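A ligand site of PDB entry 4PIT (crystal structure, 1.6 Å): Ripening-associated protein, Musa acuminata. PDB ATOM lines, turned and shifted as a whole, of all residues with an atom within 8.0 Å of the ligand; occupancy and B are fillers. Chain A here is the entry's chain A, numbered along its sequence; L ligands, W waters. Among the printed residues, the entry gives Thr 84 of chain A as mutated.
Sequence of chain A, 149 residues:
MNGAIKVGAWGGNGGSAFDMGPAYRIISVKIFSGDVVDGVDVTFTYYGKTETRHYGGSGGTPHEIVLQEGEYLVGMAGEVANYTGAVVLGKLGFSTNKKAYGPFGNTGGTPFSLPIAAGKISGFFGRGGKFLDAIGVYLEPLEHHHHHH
The side-chain carboxylate of Asp 38 sits at hydrogen-bond distance from an oxygen (O4) of the ligand (2.6 Å). O3 of the ligand lies within hydrogen-bond range of N of Gly 60. N of Val 36 lies within hydrogen-bond range of O6 of the ligand (2.9 Å). An oxygen (O6) of the ligand sits at hydrogen-bond distance from the backbone carbonyl oxygen (O) of Val 36 (3.1 Å). N of Asp 35 is in hydrogen-bond range of O5 of the ligand, 2.9 Å away. An oxygen (O6) of the ligand sits at hydrogen-bond distance from the backbone NH (N) of Gly 34 (3.3 Å).
The backbone NH (N) of Gly 34 is in hydrogen-bond range of the side-chain carboxylate (OD1) of Asp 38 (3.4 Å). O of Phe 32 sits at hydrogen-bond distance from N of Asp 38, 2.7 Å away. The backbone carbonyl oxygen of Asp 38 sits at hydrogen-bond distance from the backbone NH of Gly 57, at 2.8 Å. The side-chain carboxylate (OD2) of Asp 35 is in hydrogen-bond range of the side-chain hydroxyl (OH) of Tyr 83 (2.6 Å). O of Asp 35 sits at hydrogen-bond distance from N of Asn 106 (2.9 Å). OG1 of Thr 107 sits at hydrogen-bond distance from O of Asp 35 (2.7 Å). OD1 of Asn 106 lies close to O of Gly 34.
Merely in contact with the ligand: Phe 131, Gly 59 and Tyr 83. Hydrophobic or aromatic side chains within 4 Å of the ligand: Val 36 and Phe 131. Along chain A the residues within 4 Å of the ligand span positions 34 to 131. The nearest printed residue that does not touch the ligand is Ser 33 (4.3 Å).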
ATOM      1  N   PHE A  32      -0.815 -13.741 -20.782  1.00  0.00           N
ATOM      2  CA  PHE A  32      -1.153 -13.491 -22.194  1.00  0.00           C
ATOM      3  C   PHE A  32      -0.090 -14.098 -23.065  1.00  0.00           C
ATOM      4  O   PHE A  32       1.095 -13.770 -22.882  1.00  0.00           O
ATOM      5  CB  PHE A  32      -1.231 -11.985 -22.479  1.00  0.00           C
ATOM      6  CG  PHE A  32      -2.392 -11.272 -21.847  1.00  0.00           C
ATOM      7  CD1 PHE A  32      -2.448 -11.099 -20.475  1.00  0.00           C
ATOM      8  CD2 PHE A  32      -3.368 -10.671 -22.632  1.00  0.00           C
ATOM      9  CE1 PHE A  32      -3.506 -10.410 -19.870  1.00  0.00           C
ATOM     10  CE2 PHE A  32      -4.423  -9.961 -22.038  1.00  0.00           C
ATOM     11  CZ  PHE A  32      -4.491  -9.859 -20.653  1.00  0.00           C
ATOM     12  N   SER A  33      -0.441 -15.059 -23.920  1.00  0.00           N
ATOM     13  CA  SER A  33       0.605 -15.709 -24.710  1.00  0.00           C
ATOM     14  C   SER A  33       0.129 -16.064 -26.089  1.00  0.00           C
ATOM     15  O   SER A  33      -1.083 -16.207 -26.363  1.00  0.00           O
ATOM     16  CB  SER A  33       1.141 -16.974 -24.020  1.00  0.00           C
ATOM     17  OG  SER A  33       0.130 -17.970 -23.941  1.00  0.00           O
ATOM     18  N   GLY A  34       1.109 -16.230 -26.972  1.00  0.00           N
ATOM     19  CA  GLY A  34       0.893 -16.692 -28.329  1.00  0.00           C
ATOM     20  C   GLY A  34       2.148 -17.490 -28.667  1.00  0.00           C
ATOM     21  O   GLY A  34       2.414 -18.519 -28.034  1.00  0.00           O
ATOM     22  N   ASP A  35       2.969 -16.993 -29.604  1.00  0.00           N
ATOM     23  CA  ASP A  35       4.271 -17.595 -29.869  1.00  0.00           C
ATOM     24  C   ASP A  35       5.150 -17.491 -28.607  1.00  0.00           C
ATOM     25  O   ASP A  35       5.855 -18.445 -28.266  1.00  0.00           O
ATOM     26  CB  ASP A  35       4.985 -16.851 -30.995  1.00  0.00           C
ATOM     27  CG  ASP A  35       4.394 -17.018 -32.371  1.00  0.00           C
ATOM     28  OD1 ASP A  35       3.530 -17.895 -32.543  1.00  0.00           O
ATOM     29  OD2 ASP A  35       4.855 -16.304 -33.302  1.00  0.00           O
ATOM     30  N   VAL A  36       5.049 -16.359 -27.895  1.00  0.00           N
ATOM     31  CA  VAL A  36       5.824 -16.146 -26.658  1.00  0.00           C
ATOM     32  C   VAL A  36       4.874 -15.652 -25.566  1.00  0.00           C
ATOM     33  O   VAL A  36       3.648 -15.625 -25.766  1.00  0.00           O
ATOM     34  CB  VAL A  36       7.002 -15.146 -26.881  1.00  0.00           C
ATOM     35  CG1 VAL A  36       8.024 -15.708 -27.873  1.00  0.00           C
ATOM     36  CG2 VAL A  36       6.531 -13.739 -27.294  1.00  0.00           C
ATOM     37  N   VAL A  37       5.420 -15.218 -24.443  1.00  0.00           N
ATOM     38  CA  VAL A  37       4.602 -14.634 -23.384  1.00  0.00           C
ATOM     39  C   VAL A  37       4.561 -13.144 -23.650  1.00  0.00           C
ATOM     40  O   VAL A  37       5.596 -12.469 -23.576  1.00  0.00           O
ATOM     41  CB  VAL A  37       5.142 -14.954 -21.970  1.00  0.00           C
ATOM     42  CG1 VAL A  37       4.281 -14.264 -20.894  1.00  0.00           C
ATOM     43  CG2 VAL A  37       5.185 -16.473 -21.738  1.00  0.00           C
ATOM     44  N   ASP A  38       3.355 -12.649 -23.953  1.00  0.00           N
ATOM     45  CA  ASP A  38       3.145 -11.231 -24.246  1.00  0.00           C
ATOM     46  C   ASP A  38       3.120 -10.363 -23.005  1.00  0.00           C
ATOM     47  O   ASP A  38       3.694  -9.277 -22.990  1.00  0.00           O
ATOM     48  CB  ASP A  38       1.838 -11.059 -24.999  1.00  0.00           C
ATOM     49  CG  ASP A  38       1.931 -11.651 -26.384  1.00  0.00           C
ATOM     50  OD1 ASP A  38       1.803 -12.897 -26.508  1.00  0.00           O
ATOM     51  OD2 ASP A  38       2.111 -10.857 -27.351  1.00  0.00           O
ATOM     52  N   GLY A  39       2.480 -10.840 -21.941  1.00  0.00           N
ATOM     53  CA  GLY A  39       2.390 -10.048 -20.732  1.00  0.00           C
ATOM     54  C   GLY A  39       1.572 -10.774 -19.686  1.00  0.00           C
ATOM     55  O   GLY A  39       1.189 -11.934 -19.876  1.00  0.00           O
ATOM     56  N   GLY A  57       3.068  -6.536 -22.901  1.00  0.00           N
ATOM     57  CA  GLY A  57       2.118  -6.243 -23.968  1.00  0.00           C
ATOM     58  C   GLY A  57       0.806  -6.963 -23.743  1.00  0.00           C
ATOM     59  O   GLY A  57       0.659  -7.758 -22.809  1.00  0.00           O
ATOM     60  N   SER A  58      -0.136  -6.751 -24.678  1.00  0.00           N
ATOM     61  CA  SER A  58      -1.462  -7.349 -24.562  1.00  0.00           C
ATOM     62  C   SER A  58      -1.897  -8.103 -25.796  1.00  0.00           C
ATOM     63  O   SER A  58      -3.100  -8.389 -25.949  1.00  0.00           O
ATOM     64  CB  SER A  58      -2.486  -6.282 -24.204  1.00  0.00           C
ATOM     65  OG  SER A  58      -2.110  -5.725 -22.954  1.00  0.00           O
ATOM     66  N   GLY A  59      -0.916  -8.482 -26.620  1.00  0.00           N
ATOM     67  CA  GLY A  59      -1.150  -9.393 -27.717  1.00  0.00           C
ATOM     68  C   GLY A  59      -1.331 -10.769 -27.115  1.00  0.00           C
ATOM     69  O   GLY A  59      -1.390 -10.898 -25.876  1.00  0.00           O
ATOM     70  N   GLY A  60      -1.493 -11.771 -27.963  1.00  0.00           N
ATOM     71  CA  GLY A  60      -1.732 -13.149 -27.542  1.00  0.00           C
ATOM     72  C   GLY A  60      -3.113 -13.292 -26.960  1.00  0.00           C
ATOM     73  O   GLY A  60      -3.988 -12.455 -27.202  1.00  0.00           O
ATOM     74  N   THR A  61      -3.312 -14.393 -26.238  1.00  0.00           N
ATOM     75  CA  THR A  61      -4.591 -14.716 -25.633  1.00  0.00           C
ATOM     76  C   THR A  61      -4.400 -14.849 -24.133  1.00  0.00           C
ATOM     77  O   THR A  61      -3.411 -15.466 -23.714  1.00  0.00           O
ATOM     78  CB  THR A  61      -5.144 -16.049 -26.203  1.00  0.00           C
ATOM     79  OG1 THR A  61      -5.212 -16.012 -27.621  1.00  0.00           O
ATOM     80  CG2 THR A  61      -6.569 -16.330 -25.736  1.00  0.00           C
ATOM     81  N   TYR A  83      13.333 -14.295 -29.743  1.00  0.00           N
ATOM     82  CA  TYR A  83      12.165 -14.077 -30.596  1.00  0.00           C
ATOM     83  C   TYR A  83      12.183 -12.683 -31.151  1.00  0.00           C
ATOM     84  O   TYR A  83      12.318 -11.715 -30.400  1.00  0.00           O
ATOM     85  CB  TYR A  83      10.865 -14.311 -29.780  1.00  0.00           C
ATOM     86  CG  TYR A  83       9.580 -14.203 -30.574  1.00  0.00           C
ATOM     87  CD1 TYR A  83       9.177 -15.226 -31.422  1.00  0.00           C
ATOM     88  CD2 TYR A  83       8.723 -13.118 -30.401  1.00  0.00           C
ATOM     89  CE1 TYR A  83       7.953 -15.172 -32.101  1.00  0.00           C
ATOM     90  CE2 TYR A  83       7.507 -13.043 -31.083  1.00  0.00           C
ATOM     91  CZ  TYR A  83       7.127 -14.073 -31.929  1.00  0.00           C
ATOM     92  OH  TYR A  83       5.918 -13.998 -32.591  1.00  0.00           O
ATOM     93  N   THR A  84      12.081 -12.569 -32.481  1.00  0.00           N
ATOM     94  CA  THR A  84      12.089 -11.293 -33.206  1.00  0.00           C
ATOM     95  C   THR A  84      13.295 -10.402 -32.794  1.00  0.00           C
ATOM     96  O   THR A  84      13.132  -9.203 -32.642  1.00  0.00           O
ATOM     97  CB  THR A  84      10.739 -10.532 -33.047  1.00  0.00           C
ATOM     98  OG1 THR A  84      10.559 -10.057 -31.708  1.00  0.00           O
ATOM     99  CG2 THR A  84       9.560 -11.330 -33.540  1.00  0.00           C
ATOM    100  N   VAL A  88      13.220 -12.817 -24.528  1.00  0.00           N
ATOM    101  CA  VAL A  88      11.980 -12.620 -23.765  1.00  0.00           C
ATOM    102  C   VAL A  88      11.545 -13.910 -23.144  1.00  0.00           C
ATOM    103  O   VAL A  88      12.170 -14.952 -23.360  1.00  0.00           O
ATOM    104  CB  VAL A  88      10.864 -12.119 -24.746  1.00  0.00           C
ATOM    105  CG1 VAL A  88      11.231 -10.770 -25.395  1.00  0.00           C
ATOM    106  CG2 VAL A  88      10.556 -13.177 -25.810  1.00  0.00           C
ATOM    107  N   LEU A  89      10.416 -13.887 -22.393  1.00  0.00           N
ATOM    108  CA  LEU A  89       9.871 -15.157 -21.913  1.00  0.00           C
ATOM    109  C   LEU A  89       9.177 -15.876 -23.075  1.00  0.00           C
ATOM    110  O   LEU A  89       8.203 -15.315 -23.618  1.00  0.00           O
ATOM    111  CB  LEU A  89       8.877 -14.902 -20.800  1.00  0.00           C
ATOM    112  CG  LEU A  89       9.450 -14.770 -19.366  1.00  0.00           C
ATOM    113  CD1 LEU A  89      10.010 -16.111 -18.877  1.00  0.00           C
ATOM    114  CD2 LEU A  89      10.514 -13.687 -19.238  1.00  0.00           C
ATOM    115  N   GLY A  90       9.663 -17.067 -23.458  1.00  0.00           N
ATOM    116  CA  GLY A  90       9.057 -17.861 -24.537  1.00  0.00           C
ATOM    117  C   GLY A  90       7.902 -18.689 -23.989  1.00  0.00           C
ATOM    118  O   GLY A  90       6.937 -19.010 -24.716  1.00  0.00           O
ATOM    119  N   GLY A 105       2.683 -20.186 -23.862  1.00  0.00           N
ATOM    120  CA  GLY A 105       3.703 -19.730 -24.807  1.00  0.00           C
ATOM    121  C   GLY A 105       4.305 -20.934 -25.539  1.00  0.00           C
ATOM    122  O   GLY A 105       4.187 -22.083 -25.070  1.00  0.00           O
ATOM    123  N   ASN A 106       4.888 -20.694 -26.706  1.00  0.00           N
ATOM    124  CA  ASN A 106       5.308 -21.835 -27.531  1.00  0.00           C
ATOM    125  C   ASN A 106       6.750 -21.773 -27.999  1.00  0.00           C
ATOM    126  O   ASN A 106       7.133 -22.601 -28.824  1.00  0.00           O
ATOM    127  CB  ASN A 106       4.404 -21.902 -28.762  1.00  0.00           C
ATOM    128  CG  ASN A 106       3.009 -22.374 -28.427  1.00  0.00           C
ATOM    129  OD1 ASN A 106       2.037 -21.655 -28.574  1.00  0.00           O
ATOM    130  ND2 ASN A 106       2.934 -23.622 -28.082  1.00  0.00           N
ATOM    131  N   THR A 107       7.534 -20.814 -27.510  1.00  0.00           N
ATOM    132  CA  THR A 107       8.903 -20.743 -27.994  1.00  0.00           C
ATOM    133  C   THR A 107       9.876 -21.234 -26.929  1.00  0.00           C
ATOM    134  O   THR A 107       9.999 -20.673 -25.823  1.00  0.00           O
ATOM    135  CB  THR A 107       9.225 -19.345 -28.455  1.00  0.00           C
ATOM    136  OG1 THR A 107       8.247 -18.884 -29.402  1.00  0.00           O
ATOM    137  CG2 THR A 107      10.593 -19.292 -29.172  1.00  0.00           C
ATOM    138  N   LYS A 130       6.773  -4.865 -25.946  1.00  0.00           N
ATOM    139  CA  LYS A 130       5.705  -5.479 -26.729  1.00  0.00           C
ATOM    140  C   LYS A 130       5.411  -6.844 -26.128  1.00  0.00           C
ATOM    141  O   LYS A 130       4.276  -7.311 -26.183  1.00  0.00           O
ATOM    142  CB  LYS A 130       6.112  -5.619 -28.214  1.00  0.00           C
ATOM    143  CG  LYS A 130       4.988  -6.124 -29.102  1.00  0.00           C
ATOM    144  CD  LYS A 130       5.421  -6.060 -30.548  1.00  0.00           C
ATOM    145  CE  LYS A 130       4.419  -6.723 -31.462  1.00  0.00           C
ATOM    146  NZ  LYS A 130       3.162  -5.934 -31.548  1.00  0.00           N
ATOM    147  N   PHE A 131       6.439  -7.493 -25.554  1.00  0.00           N
ATOM    148  CA  PHE A 131       6.300  -8.799 -24.922  1.00  0.00           C
ATOM    149  C   PHE A 131       6.804  -8.743 -23.486  1.00  0.00           C
ATOM    150  O   PHE A 131       7.115  -7.664 -22.964  1.00  0.00           O
ATOM    151  CB  PHE A 131       6.998  -9.920 -25.729  1.00  0.00           C
ATOM    152  CG  PHE A 131       6.716  -9.883 -27.220  1.00  0.00           C
ATOM    153  CD1 PHE A 131       5.415  -9.999 -27.684  1.00  0.00           C
ATOM    154  CD2 PHE A 131       7.748  -9.689 -28.133  1.00  0.00           C
ATOM    155  CE1 PHE A 131       5.146 -10.006 -29.054  1.00  0.00           C
ATOM    156  CE2 PHE A 131       7.473  -9.654 -29.521  1.00  0.00           C
ATOM    157  CZ  PHE A 131       6.166  -9.756 -29.961  1.00  0.00           C
HETATM  158  C1  LIG L   1       1.341 -14.697 -32.238  1.00  0.00           C
HETATM  159  C2  LIG L   1      -0.022 -14.138 -31.804  1.00  0.00           C
HETATM  160  C3  LIG L   1       0.120 -12.714 -31.277  1.00  0.00           C
HETATM  161  C4  LIG L   1       1.174 -12.649 -30.174  1.00  0.00           C
HETATM  162  C5  LIG L   1       2.495 -13.256 -30.658  1.00  0.00           C
HETATM  163  C6  LIG L   1       3.545 -13.346 -29.557  1.00  0.00           C
HETATM  164  O1  LIG L   1       1.784 -14.015 -33.407  1.00  0.00           O
HETATM  165  O2  LIG L   1      -0.597 -14.998 -30.825  1.00  0.00           O
HETATM  166  O3  LIG L   1      -1.114 -12.195 -30.794  1.00  0.00           O
HETATM  167  O4  LIG L   1       1.353 -11.294 -29.789  1.00  0.00           O
HETATM  168  O5  LIG L   1       2.293 -14.594 -31.151  1.00  0.00           O
HETATM  169  O6  LIG L   1       3.163 -14.227 -28.499  1.00  0.00           O
HETATM  170  O   HOH W   1       3.359 -12.353 -35.261  1.00  0.00           O
HETATM  171  O   HOH W   2       0.039 -18.160 -31.194  1.00  0.00           O
HETATM  172  O   HOH W   3       1.868  -9.304 -31.524  1.00  0.00           O
